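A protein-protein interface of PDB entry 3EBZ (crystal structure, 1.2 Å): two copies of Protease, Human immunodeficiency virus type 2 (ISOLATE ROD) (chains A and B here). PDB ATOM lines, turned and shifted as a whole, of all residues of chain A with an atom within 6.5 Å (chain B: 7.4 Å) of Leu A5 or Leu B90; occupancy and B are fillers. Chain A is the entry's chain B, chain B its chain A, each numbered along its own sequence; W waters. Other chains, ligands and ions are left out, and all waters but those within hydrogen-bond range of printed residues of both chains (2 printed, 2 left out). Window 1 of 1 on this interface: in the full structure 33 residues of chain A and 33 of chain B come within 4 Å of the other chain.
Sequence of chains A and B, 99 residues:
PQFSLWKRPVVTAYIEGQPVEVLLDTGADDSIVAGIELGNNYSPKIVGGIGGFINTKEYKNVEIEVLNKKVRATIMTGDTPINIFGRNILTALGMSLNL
Water W2 lies within hydrogen-bond range of OXT of Leu A99 and O of Gly B94. Water W1 lies within hydrogen-bond range of O of Gly B27 (2.9 Å), OD1 of Asp B29 (3.0 Å) and NE of Arg A8 (3.3 Å).
Printed residues of chain B within 4 Å of Leu A5: Thr B26 (3.8 Å), Arg B87 (2.9 Å), Leu B90 (3.99 Å), Thr B91 (3.2 Å) and Met B95 (3.7 Å). Printed residues of chain A within 4 Å of Leu B90: Leu A5. Of the printed residues of chain B, Pro A9 touches Thr B26 and Arg B87. Printed residues of chain B within 4 Å of Leu A99: Leu B67 (3.7 Å), Leu B93 (3.2 Å) and Met B95 (3.9 Å). Of the printed residues of chain B, Thr A26 touches Leu B24 (2.8 Å), Asp B25 (3.5 Å), Thr B26 (2.9 Å) and Leu B97 (3.9 Å). Printed residues of chain B within 4 Å of Ser A4: Thr B91 (3.7 Å) and Met B95 (3.8 Å). Of the printed residues of chain B, Leu A97 touches Leu B24 (3.9 Å), Thr B26 (3.7 Å), Met B95 (3.9 Å) and Ser B96 (3.4 Å). Gly B86 touches none of the printed residues of chain A. Val B66 touches none of the printed residues of chain A. The nearest printed residue of chain B that does not touch Leu A5 is Leu B97 (4.2 Å).
The guanidinium group (NH1) of Arg B87 is in hydrogen-bond range of the backbone carbonyl oxygen (O) of Leu A5, at 2.9 Å. O of Leu B24 lies within hydrogen-bond range of OG1 of Thr A26, 2.8 Å away. The side-chain carboxylate (OD2) of Asp B29 is in salt-bridge range of the guanidinium group (NH2) of Arg A8, at 2.9 Å. The backbone NH (N) of Phe A3 sits at hydrogen-bond distance from the backbone carbonyl oxygen (O) of Leu B97 (2.7 Å). OG1 of Thr B26 is in hydrogen-bond range of O of Leu A24 (2.7 Å). The backbone NH of Thr B26 is in hydrogen-bond range of the side-chain hydroxyl of Thr A26 (2.9 Å). The backbone carbonyl oxygen (O) of Trp A6 lies within hydrogen-bond range of the guanidinium group (NH1) of Arg B87, at 3.3 Å.
The backbone carbonyl oxygen of Ala B28 sits at hydrogen-bond distance from the backbone NH of Arg B87. O of Arg B87 is in hydrogen-bond range of OG1 of Thr B91 (2.8 Å). O of Leu B90 is in hydrogen-bond range of N of Met B95. The side-chain carboxylate (OD1) of Asp B25 sits at hydrogen-bond distance from the backbone NH (N) of Gly B27, 2.8 Å away. The side-chain hydroxyl (OG1) of Thr B91 lies within hydrogen-bond range of the backbone carbonyl oxygen (O) of Asn B88 (3.2 Å). The backbone carbonyl oxygen (O) of Pro A9 is in hydrogen-bond range of the backbone NH (N) of Leu A24 (2.9 Å).
Among the printed residues, pairs that only touch across the chains: Phe A3 with Ser B96 (3.4 Å), Ser A4 with Thr B91 (3.7 Å), Ser A4 with Met B95 (3.8 Å), Leu A5 with Thr B26 (3.8 Å), Leu A5 with Leu B90 (3.99 Å), Leu A5 with Thr B91 (3.2 Å), Leu A5 with Met B95 (3.7 Å), Trp A6 with Thr B91 (3.5 Å), Lys A7 with Arg B87 (3.4 Å), Arg A8 with Arg B87 (3.5 Å), Pro A9 with Thr B26 (3.6 Å), Pro A9 with Arg B87 (3.8 Å), Leu A24 with Leu B97 (3.8 Å), Thr A26 with Asp B25 (3.5 Å), Thr A26 with Leu B97 (3.9 Å), Leu A97 with Leu B24 (3.9 Å), Leu A97 with Thr B26 (3.7 Å), Leu A97 with Met B95 (3.9 Å), Leu A97 with Ser B96 (3.4 Å), Leu A99 with Leu B67 (3.7 Å), Leu A99 with Leu B93 (3.2 Å) and Leu A99 with Met B95 (3.9 Å).
Of the 23 printed residues of chain B, 12 touch a printed residue of chain A. Hydrophobic or aromatic side chains of chain B within 4 Å of the printed part of chain A: Leu B24, Leu B67, Leu B90, Met B95 and Leu B97. Along chain B the printed residues that touch a printed residue of chain A span positions 24 to 97. Along chain A the printed residues that touch a printed residue of chain B span positions 3 to 99. Among the printed residues, 29 pairs touch across the chains. Among the printed residues, Asp or Glu carboxylates within 4 Å of a Lys or Arg side-chain nitrogen of the other chain: Arg A8 with Asp B29 (2.9 Å).
Leu A24 touches Thr B26, and with the chains exchanged Thr A26 touches Leu B24. Leu A24 touches Leu B97, and with the chains exchanged Leu A97 touches Leu B24. Thr B26 touches its own counterpart, Thr A26. Thr A26 touches Leu B97, and with the chains exchanged Leu A97 touches Thr B26. Of the 29 pairs that touch across the chains among the printed residues, 7 have their exchanged pair printed and touching as well.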
ATOM      1  N   PHE A   3       4.131  22.073 -20.467  1.00  0.00           N
ATOM      2  CA  PHE A   3       3.638  20.752 -20.857  1.00  0.00           C
ATOM      3  C   PHE A   3       2.847  20.863 -22.149  1.00  0.00           C
ATOM      4  O   PHE A   3       1.794  21.503 -22.217  1.00  0.00           O
ATOM      5  CB  PHE A   3       2.759  20.189 -19.733  1.00  0.00           C
ATOM      6  CG  PHE A   3       3.519  19.920 -18.441  1.00  0.00           C
ATOM      7  CD1 PHE A   3       3.642  20.947 -17.524  1.00  0.00           C
ATOM      8  CD2 PHE A   3       4.096  18.683 -18.210  1.00  0.00           C
ATOM      9  CE1 PHE A   3       4.346  20.774 -16.343  1.00  0.00           C
ATOM     10  CE2 PHE A   3       4.795  18.515 -17.016  1.00  0.00           C
ATOM     11  CZ  PHE A   3       4.934  19.561 -16.121  1.00  0.00           C
ATOM     12  N   SER A   4       3.375  20.293 -23.230  1.00  0.00           N
ATOM     13  CA  SER A   4       2.739  20.399 -24.547  1.00  0.00           C
ATOM     14  C   SER A   4       1.613  19.419 -24.840  1.00  0.00           C
ATOM     15  O   SER A   4       0.965  19.527 -25.867  1.00  0.00           O
ATOM     16  CB  SER A   4       3.864  20.261 -25.565  1.00  0.00           C
ATOM     17  OG  SER A   4       4.582  21.519 -25.506  1.00  0.00           O
ATOM     18  N   LEU A   5       1.372  18.501 -23.912  1.00  0.00           N
ATOM     19  CA  LEU A   5       0.194  17.642 -23.873  1.00  0.00           C
ATOM     20  C   LEU A   5       0.174  16.561 -24.935  1.00  0.00           C
ATOM     21  O   LEU A   5      -0.790  15.779 -25.001  1.00  0.00           O
ATOM     22  CB  LEU A   5      -1.094  18.484 -23.895  1.00  0.00           C
ATOM     23  CG  LEU A   5      -1.170  19.546 -22.784  1.00  0.00           C
ATOM     24  CD1 LEU A   5      -2.428  20.387 -23.015  1.00  0.00           C
ATOM     25  CD2 LEU A   5      -1.153  18.912 -21.416  1.00  0.00           C
ATOM     26  N   TRP A   6       1.244  16.403 -25.733  1.00  0.00           N
ATOM     27  CA  TRP A   6       1.365  15.226 -26.597  1.00  0.00           C
ATOM     28  C   TRP A   6       1.580  13.952 -25.778  1.00  0.00           C
ATOM     29  O   TRP A   6       1.211  12.888 -26.250  1.00  0.00           O
ATOM     30  CB  TRP A   6       2.470  15.468 -27.610  1.00  0.00           C
ATOM     31  CG  TRP A   6       2.211  16.635 -28.513  1.00  0.00           C
ATOM     32  CD1 TRP A   6       2.762  17.884 -28.443  1.00  0.00           C
ATOM     33  CD2 TRP A   6       1.320  16.627 -29.648  1.00  0.00           C
ATOM     34  NE1 TRP A   6       2.257  18.667 -29.473  1.00  0.00           N
ATOM     35  CE2 TRP A   6       1.377  17.913 -30.213  1.00  0.00           C
ATOM     36  CE3 TRP A   6       0.479  15.653 -30.223  1.00  0.00           C
ATOM     37  CZ2 TRP A   6       0.635  18.274 -31.336  1.00  0.00           C
ATOM     38  CZ3 TRP A   6      -0.261  16.013 -31.342  1.00  0.00           C
ATOM     39  CH2 TRP A   6      -0.167  17.305 -31.865  1.00  0.00           C
ATOM     40  N   LYS A   7       2.171  14.061 -24.586  1.00  0.00           N
ATOM     41  CA  LYS A   7       2.288  13.057 -23.564  1.00  0.00           C
ATOM     42  C   LYS A   7       1.472  13.515 -22.365  1.00  0.00           C
ATOM     43  O   LYS A   7       1.182  14.697 -22.161  1.00  0.00           O
ATOM     44  CB  LYS A   7       3.742  12.795 -23.171  1.00  0.00           C
ATOM     45  CG  LYS A   7       4.516  13.950 -22.514  1.00  0.00           C
ATOM     46  CD  LYS A   7       5.939  13.636 -22.104  1.00  0.00           C
ATOM     47  CE  LYS A   7       6.701  14.824 -21.559  1.00  0.00           C
ATOM     48  NZ  LYS A   7       8.130  14.545 -21.134  1.00  0.00           N
ATOM     49  N   ARG A   8       1.078  12.577 -21.515  1.00  0.00           N
ATOM     50  CA  ARG A   8       0.415  12.941 -20.262  1.00  0.00           C
ATOM     51  C   ARG A   8       1.285  13.893 -19.457  1.00  0.00           C
ATOM     52  O   ARG A   8       2.520  13.626 -19.372  1.00  0.00           O
ATOM     53  CB  ARG A   8       0.156  11.703 -19.401  1.00  0.00           C
ATOM     54  CG  ARG A   8      -0.901  10.763 -19.927  1.00  0.00           C
ATOM     55  CD  ARG A   8      -1.158   9.656 -18.877  1.00  0.00           C
ATOM     56  NE  ARG A   8      -2.202   8.751 -19.396  1.00  0.00           N
ATOM     57  CZ  ARG A   8      -2.550   7.583 -18.888  1.00  0.00           C
ATOM     58  NH1 ARG A   8      -1.905   7.144 -17.790  1.00  0.00           N
ATOM     59  NH2 ARG A   8      -3.509   6.862 -19.456  1.00  0.00           N
ATOM     60  N   PRO A   9       0.743  14.941 -18.853  1.00  0.00           N
ATOM     61  CA  PRO A   9       1.557  15.789 -17.988  1.00  0.00           C
ATOM     62  C   PRO A   9       1.696  15.209 -16.588  1.00  0.00           C
ATOM     63  O   PRO A   9       1.099  15.641 -15.635  1.00  0.00           O
ATOM     64  CB  PRO A   9       0.746  17.106 -17.990  1.00  0.00           C
ATOM     65  CG  PRO A   9      -0.714  16.691 -18.156  1.00  0.00           C
ATOM     66  CD  PRO A   9      -0.614  15.508 -19.086  1.00  0.00           C
ATOM     67  N   LEU A  24      -1.087  16.091 -13.751  1.00  0.00           N
ATOM     68  CA  LEU A  24      -1.600  17.451 -13.622  1.00  0.00           C
ATOM     69  C   LEU A  24      -2.904  17.530 -14.402  1.00  0.00           C
ATOM     70  O   LEU A  24      -2.883  17.365 -15.624  1.00  0.00           O
ATOM     71  CB  LEU A  24      -0.558  18.456 -14.110  1.00  0.00           C
ATOM     72  CG  LEU A  24       0.812  18.340 -13.427  1.00  0.00           C
ATOM     73  CD1 LEU A  24       1.783  19.364 -14.055  1.00  0.00           C
ATOM     74  CD2 LEU A  24       0.755  18.520 -11.926  1.00  0.00           C
ATOM     75  N   THR A  26      -6.412  19.420 -15.173  1.00  0.00           N
ATOM     76  CA  THR A  26      -7.222  20.597 -15.233  1.00  0.00           C
ATOM     77  C   THR A  26      -8.713  20.267 -15.180  1.00  0.00           C
ATOM     78  O   THR A  26      -9.468  21.159 -14.830  1.00  0.00           O
ATOM     79  CB  THR A  26      -6.939  21.466 -16.444  1.00  0.00           C
ATOM     80  OG1 THR A  26      -7.204  20.718 -17.646  1.00  0.00           O
ATOM     81  CG2 THR A  26      -5.516  21.963 -16.529  1.00  0.00           C
ATOM     82  N   LEU A  97      -3.594  27.195 -18.403  1.00  0.00           N
ATOM     83  CA  LEU A  97      -3.779  26.557 -19.706  1.00  0.00           C
ATOM     84  C   LEU A  97      -3.836  27.686 -20.735  1.00  0.00           C
ATOM     85  O   LEU A  97      -4.541  28.672 -20.512  1.00  0.00           O
ATOM     86  CB  LEU A  97      -5.008  25.711 -19.706  1.00  0.00           C
ATOM     87  CG  LEU A  97      -5.429  24.612 -20.600  1.00  0.00           C
ATOM     88  CD1 LEU A  97      -4.402  23.503 -20.681  1.00  0.00           C
ATOM     89  CD2 LEU A  97      -6.790  24.043 -20.113  1.00  0.00           C
ATOM     90  N   LEU A  99      -3.415  28.973 -25.110  1.00  0.00           N
ATOM     91  CA  LEU A  99      -3.586  28.790 -26.526  1.00  0.00           C
ATOM     92  C   LEU A  99      -3.236  30.119 -27.204  1.00  0.00           C
ATOM     93  O   LEU A  99      -3.715  31.171 -26.711  1.00  0.00           O
ATOM     94  CB  LEU A  99      -5.033  28.439 -26.828  1.00  0.00           C
ATOM     95  CG  LEU A  99      -5.419  27.650 -28.048  1.00  0.00           C
ATOM     96  CD1 LEU A  99      -6.910  27.836 -28.317  1.00  0.00           C
ATOM     97  CD2 LEU A  99      -4.634  28.010 -29.298  1.00  0.00           C
ATOM     98  OXT LEU A  99      -2.496  30.056 -28.207  1.00  0.00           O
ATOM     99  N   LEU B  23     -15.305  20.465 -21.058  1.00  0.00           N
ATOM    100  CA  LEU B  23     -14.269  20.742 -20.076  1.00  0.00           C
ATOM    101  C   LEU B  23     -12.915  20.519 -20.729  1.00  0.00           C
ATOM    102  O   LEU B  23     -12.670  19.425 -21.278  1.00  0.00           O
ATOM    103  CB  LEU B  23     -14.461  19.776 -18.919  1.00  0.00           C
ATOM    104  CG  LEU B  23     -13.480  19.781 -17.748  1.00  0.00           C
ATOM    105  CD1 LEU B  23     -13.522  21.115 -17.015  1.00  0.00           C
ATOM    106  CD2 LEU B  23     -13.791  18.663 -16.799  1.00  0.00           C
ATOM    107  N   LEU B  24     -11.991  21.478 -20.676  1.00  0.00           N
ATOM    108  CA  LEU B  24     -10.659  21.330 -21.262  1.00  0.00           C
ATOM    109  C   LEU B  24      -9.786  20.601 -20.256  1.00  0.00           C
ATOM    110  O   LEU B  24      -9.419  21.183 -19.229  1.00  0.00           O
ATOM    111  CB  LEU B  24     -10.148  22.705 -21.607  1.00  0.00           C
ATOM    112  CG  LEU B  24     -11.012  23.581 -22.519  1.00  0.00           C
ATOM    113  CD1 LEU B  24     -10.428  24.995 -22.625  1.00  0.00           C
ATOM    114  CD2 LEU B  24     -11.207  22.948 -23.887  1.00  0.00           C
ATOM    115  N   ASP B  25      -9.470  19.336 -20.525  1.00  0.00           N
ATOM    116  CA  ASP B  25      -9.008  18.427 -19.495  1.00  0.00           C
ATOM    117  C   ASP B  25      -7.654  17.804 -19.830  1.00  0.00           C
ATOM    118  O   ASP B  25      -7.556  16.861 -20.599  1.00  0.00           O
ATOM    119  CB  ASP B  25     -10.037  17.324 -19.349  1.00  0.00           C
ATOM    120  CG  ASP B  25      -9.786  16.528 -18.063  1.00  0.00           C
ATOM    121  OD1 ASP B  25      -8.710  16.726 -17.460  1.00  0.00           O
ATOM    122  OD2 ASP B  25     -10.710  15.768 -17.713  1.00  0.00           O
ATOM    123  N   THR B  26      -6.573  18.308 -19.212  1.00  0.00           N
ATOM    124  CA  THR B  26      -5.254  17.729 -19.381  1.00  0.00           C
ATOM    125  C   THR B  26      -5.098  16.331 -18.785  1.00  0.00           C
ATOM    126  O   THR B  26      -4.193  15.624 -19.148  1.00  0.00           O
ATOM    127  CB  THR B  26      -4.155  18.633 -18.813  1.00  0.00           C
ATOM    128  OG1 THR B  26      -4.349  18.750 -17.433  1.00  0.00           O
ATOM    129  CG2 THR B  26      -4.166  20.039 -19.436  1.00  0.00           C
ATOM    130  N   GLY B  27      -6.025  15.967 -17.882  1.00  0.00           N
ATOM    131  CA  GLY B  27      -6.015  14.666 -17.277  1.00  0.00           C
ATOM    132  C   GLY B  27      -6.700  13.566 -18.053  1.00  0.00           C
ATOM    133  O   GLY B  27      -6.814  12.424 -17.576  1.00  0.00           O
ATOM    134  N   ALA B  28      -7.210  13.871 -19.228  1.00  0.00           N
ATOM    135  CA  ALA B  28      -7.890  12.950 -20.103  1.00  0.00           C
ATOM    136  C   ALA B  28      -7.048  12.678 -21.357  1.00  0.00           C
ATOM    137  O   ALA B  28      -6.703  13.624 -22.049  1.00  0.00           O
ATOM    138  CB  ALA B  28      -9.243  13.489 -20.552  1.00  0.00           C
ATOM    139  N   ASP B  29      -6.731  11.462 -21.689  1.00  0.00           N
ATOM    140  CA  ASP B  29      -5.992  11.186 -22.891  1.00  0.00           C
ATOM    141  C   ASP B  29      -6.828  11.546 -24.140  1.00  0.00           C
ATOM    142  O   ASP B  29      -6.288  12.074 -25.135  1.00  0.00           O
ATOM    143  CB  ASP B  29      -5.616   9.723 -22.992  1.00  0.00           C
ATOM    144  CG  ASP B  29      -4.655   9.173 -21.985  1.00  0.00           C
ATOM    145  OD1 ASP B  29      -3.886   9.951 -21.411  1.00  0.00           O
ATOM    146  OD2 ASP B  29      -4.703   7.931 -21.853  1.00  0.00           O
ATOM    147  N   SER B  31     -11.174  12.230 -25.704  1.00  0.00           N
ATOM    148  CA  SER B  31     -12.341  13.075 -25.525  1.00  0.00           C
ATOM    149  C   SER B  31     -13.607  12.244 -25.526  1.00  0.00           C
ATOM    150  O   SER B  31     -13.758  11.271 -26.269  1.00  0.00           O
ATOM    151  CB  SER B  31     -12.342  14.107 -26.662  1.00  0.00           C
ATOM    152  OG  SER B  31     -11.197  14.951 -26.577  1.00  0.00           O
ATOM    153  N   VAL B  66     -14.039  24.854 -31.772  1.00  0.00           N
ATOM    154  CA  VAL B  66     -13.896  25.262 -30.369  1.00  0.00           C
ATOM    155  C   VAL B  66     -12.781  26.291 -30.323  1.00  0.00           C
ATOM    156  O   VAL B  66     -11.833  26.177 -31.118  1.00  0.00           O
ATOM    157  CB  VAL B  66     -13.673  24.003 -29.517  1.00  0.00           C
ATOM    158  CG1 VAL B  66     -12.320  23.376 -29.881  1.00  0.00           C
ATOM    159  CG2 VAL B  66     -13.808  24.323 -28.028  1.00  0.00           C
ATOM    160  N   LEU B  67     -12.867  27.266 -29.438  1.00  0.00           N
ATOM    161  CA  LEU B  67     -11.891  28.349 -29.258  1.00  0.00           C
ATOM    162  C   LEU B  67     -11.487  29.044 -30.540  1.00  0.00           C
ATOM    163  O   LEU B  67     -10.335  29.355 -30.829  1.00  0.00           O
ATOM    164  CB  LEU B  67     -10.655  27.854 -28.488  1.00  0.00           C
ATOM    165  CG  LEU B  67     -10.993  27.471 -27.036  1.00  0.00           C
ATOM    166  CD1 LEU B  67      -9.873  26.693 -26.388  1.00  0.00           C
ATOM    167  CD2 LEU B  67     -11.338  28.729 -26.240  1.00  0.00           C
ATOM    168  N   PHE B  85     -12.978  17.402 -23.371  1.00  0.00           N
ATOM    169  CA  PHE B  85     -12.042  17.537 -24.441  1.00  0.00           C
ATOM    170  C   PHE B  85     -10.653  17.280 -23.821  1.00  0.00           C
ATOM    171  O   PHE B  85     -10.107  18.113 -23.086  1.00  0.00           O
ATOM    172  CB  PHE B  85     -12.099  18.891 -25.150  1.00  0.00           C
ATOM    173  CG  PHE B  85     -13.199  18.972 -26.199  1.00  0.00           C
ATOM    174  CD1 PHE B  85     -13.203  20.090 -27.042  1.00  0.00           C
ATOM    175  CD2 PHE B  85     -14.180  18.024 -26.398  1.00  0.00           C
ATOM    176  CE1 PHE B  85     -14.140  20.243 -28.029  1.00  0.00           C
ATOM    177  CE2 PHE B  85     -15.117  18.184 -27.391  1.00  0.00           C
ATOM    178  CZ  PHE B  85     -15.106  19.288 -28.215  1.00  0.00           C
ATOM    179  N   GLY B  86     -10.159  16.066 -24.150  1.00  0.00           N
ATOM    180  CA  GLY B  86      -8.872  15.632 -23.629  1.00  0.00           C
ATOM    181  C   GLY B  86      -7.729  16.008 -24.574  1.00  0.00           C
ATOM    182  O   GLY B  86      -7.870  16.775 -25.512  1.00  0.00           O
ATOM    183  N   ARG B  87      -6.580  15.446 -24.258  1.00  0.00           N
ATOM    184  CA  ARG B  87      -5.345  15.882 -24.886  1.00  0.00           C
ATOM    185  C   ARG B  87      -5.369  15.684 -26.383  1.00  0.00           C
ATOM    186  O   ARG B  87      -4.685  16.456 -27.079  1.00  0.00           O
ATOM    187  CB  ARG B  87      -4.152  15.132 -24.268  1.00  0.00           C
ATOM    188  CG  ARG B  87      -3.892  15.445 -22.818  1.00  0.00           C
ATOM    189  CD  ARG B  87      -2.580  14.888 -22.288  1.00  0.00           C
ATOM    190  NE  ARG B  87      -2.602  13.421 -22.339  1.00  0.00           N
ATOM    191  CZ  ARG B  87      -2.082  12.593 -23.232  1.00  0.00           C
ATOM    192  NH1 ARG B  87      -1.375  13.069 -24.242  1.00  0.00           N
ATOM    193  NH2 ARG B  87      -2.223  11.288 -23.128  1.00  0.00           N
ATOM    194  N   ASN B  88      -6.104  14.737 -26.943  1.00  0.00           N
ATOM    195  CA  ASN B  88      -6.065  14.592 -28.388  1.00  0.00           C
ATOM    196  C   ASN B  88      -6.593  15.849 -29.060  1.00  0.00           C
ATOM    197  O   ASN B  88      -6.114  16.237 -30.129  1.00  0.00           O
ATOM    198  CB  ASN B  88      -6.879  13.363 -28.812  1.00  0.00           C
ATOM    199  CG  ASN B  88      -8.377  13.511 -28.616  1.00  0.00           C
ATOM    200  OD1 ASN B  88      -8.847  13.773 -27.504  1.00  0.00           O
ATOM    201  ND2 ASN B  88      -9.110  13.365 -29.723  1.00  0.00           N
ATOM    202  N   ILE B  89      -7.586  16.488 -28.442  1.00  0.00           N
ATOM    203  CA  ILE B  89      -8.098  17.759 -28.974  1.00  0.00           C
ATOM    204  C   ILE B  89      -7.225  18.931 -28.524  1.00  0.00           C
ATOM    205  O   ILE B  89      -6.953  19.821 -29.340  1.00  0.00           O
ATOM    206  CB  ILE B  89      -9.581  17.930 -28.640  1.00  0.00           C
ATOM    207  CG1 ILE B  89     -10.454  16.938 -29.456  1.00  0.00           C
ATOM    208  CG2 ILE B  89     -10.062  19.365 -28.861  1.00  0.00           C
ATOM    209  CD1 ILE B  89     -11.916  16.857 -29.152  1.00  0.00           C
ATOM    210  N   LEU B  90      -6.798  18.954 -27.258  1.00  0.00           N
ATOM    211  CA  LEU B  90      -5.982  20.110 -26.819  1.00  0.00           C
ATOM    212  C   LEU B  90      -4.744  20.266 -27.658  1.00  0.00           C
ATOM    213  O   LEU B  90      -4.360  21.398 -28.014  1.00  0.00           O
ATOM    214  CB  LEU B  90      -5.661  20.001 -25.325  1.00  0.00           C
ATOM    215  CG  LEU B  90      -6.846  19.762 -24.379  1.00  0.00           C
ATOM    216  CD1 LEU B  90      -6.358  19.712 -22.959  1.00  0.00           C
ATOM    217  CD2 LEU B  90      -7.951  20.817 -24.580  1.00  0.00           C
ATOM    218  N   THR B  91      -4.068  19.177 -27.972  1.00  0.00           N
ATOM    219  CA  THR B  91      -2.896  19.240 -28.822  1.00  0.00           C
ATOM    220  C   THR B  91      -3.229  19.677 -30.232  1.00  0.00           C
ATOM    221  O   THR B  91      -2.465  20.363 -30.891  1.00  0.00           O
ATOM    222  CB  THR B  91      -2.160  17.887 -28.944  1.00  0.00           C
ATOM    223  OG1 THR B  91      -3.067  16.854 -29.362  1.00  0.00           O
ATOM    224  CG2 THR B  91      -1.547  17.443 -27.617  1.00  0.00           C
ATOM    225  N   ALA B  92      -4.361  19.295 -30.775  1.00  0.00           N
ATOM    226  CA  ALA B  92      -4.732  19.758 -32.108  1.00  0.00           C
ATOM    227  C   ALA B  92      -4.974  21.256 -32.108  1.00  0.00           C
ATOM    228  O   ALA B  92      -4.795  21.907 -33.119  1.00  0.00           O
ATOM    229  CB  ALA B  92      -5.982  19.062 -32.568  1.00  0.00           C
ATOM    230  N   LEU B  93      -5.400  21.790 -30.964  1.00  0.00           N
ATOM    231  CA  LEU B  93      -5.645  23.210 -30.909  1.00  0.00           C
ATOM    232  C   LEU B  93      -4.363  23.967 -30.621  1.00  0.00           C
ATOM    233  O   LEU B  93      -4.456  25.179 -30.774  1.00  0.00           O
ATOM    234  CB  LEU B  93      -6.599  23.564 -29.777  1.00  0.00           C
ATOM    235  CG  LEU B  93      -7.984  22.930 -29.916  1.00  0.00           C
ATOM    236  CD1 LEU B  93      -8.715  23.040 -28.613  1.00  0.00           C
ATOM    237  CD2 LEU B  93      -8.760  23.659 -30.987  1.00  0.00           C
ATOM    238  N   GLY B  94      -3.297  23.304 -30.219  1.00  0.00           N
ATOM    239  CA  GLY B  94      -2.029  23.922 -29.864  1.00  0.00           C
ATOM    240  C   GLY B  94      -2.015  24.457 -28.451  1.00  0.00           C
ATOM    241  O   GLY B  94      -1.261  25.390 -28.120  1.00  0.00           O
ATOM    242  N   MET B  95      -2.816  23.872 -27.571  1.00  0.00           N
ATOM    243  CA  MET B  95      -2.849  24.272 -26.172  1.00  0.00           C
ATOM    244  C   MET B  95      -1.696  23.728 -25.347  1.00  0.00           C
ATOM    245  O   MET B  95      -1.225  22.629 -25.649  1.00  0.00           O
ATOM    246  CB  MET B  95      -4.112  23.746 -25.488  1.00  0.00           C
ATOM    247  CG  MET B  95      -5.383  24.268 -26.091  1.00  0.00           C
ATOM    248  SD  MET B  95      -6.742  24.357 -24.923  1.00  0.00           S
ATOM    249  CE  MET B  95      -6.391  25.932 -24.135  1.00  0.00           C
ATOM    250  N   SER B  96      -1.285  24.456 -24.319  1.00  0.00           N
ATOM    251  CA  SER B  96      -0.247  23.990 -23.422  1.00  0.00           C
ATOM    252  C   SER B  96      -0.613  24.301 -21.963  1.00  0.00           C
ATOM    253  O   SER B  96      -1.426  25.180 -21.705  1.00  0.00           O
ATOM    254  CB  SER B  96       1.120  24.607 -23.712  1.00  0.00           C
ATOM    255  OG  SER B  96       1.074  26.031 -23.632  1.00  0.00           O
ATOM    256  N   LEU B  97      -0.003  23.526 -21.080  1.00  0.00           N
ATOM    257  CA  LEU B  97      -0.177  23.699 -19.640  1.00  0.00           C
ATOM    258  C   LEU B  97       1.139  24.249 -19.125  1.00  0.00           C
ATOM    259  O   LEU B  97       2.195  23.639 -19.389  1.00  0.00           O
ATOM    260  CB  LEU B  97      -0.620  22.357 -19.070  1.00  0.00           C
ATOM    261  CG  LEU B  97      -0.680  22.316 -17.554  1.00  0.00           C
ATOM    262  CD1 LEU B  97      -1.858  23.166 -17.142  1.00  0.00           C
ATOM    263  CD2 LEU B  97      -0.748  20.851 -17.104  1.00  0.00           C
HETATM  264  O   HOH W   1      -4.821  10.631 -18.658  1.00  0.00           O
HETATM  265  O   HOH W   2      -0.923  28.112 -29.345  1.00  0.00           O
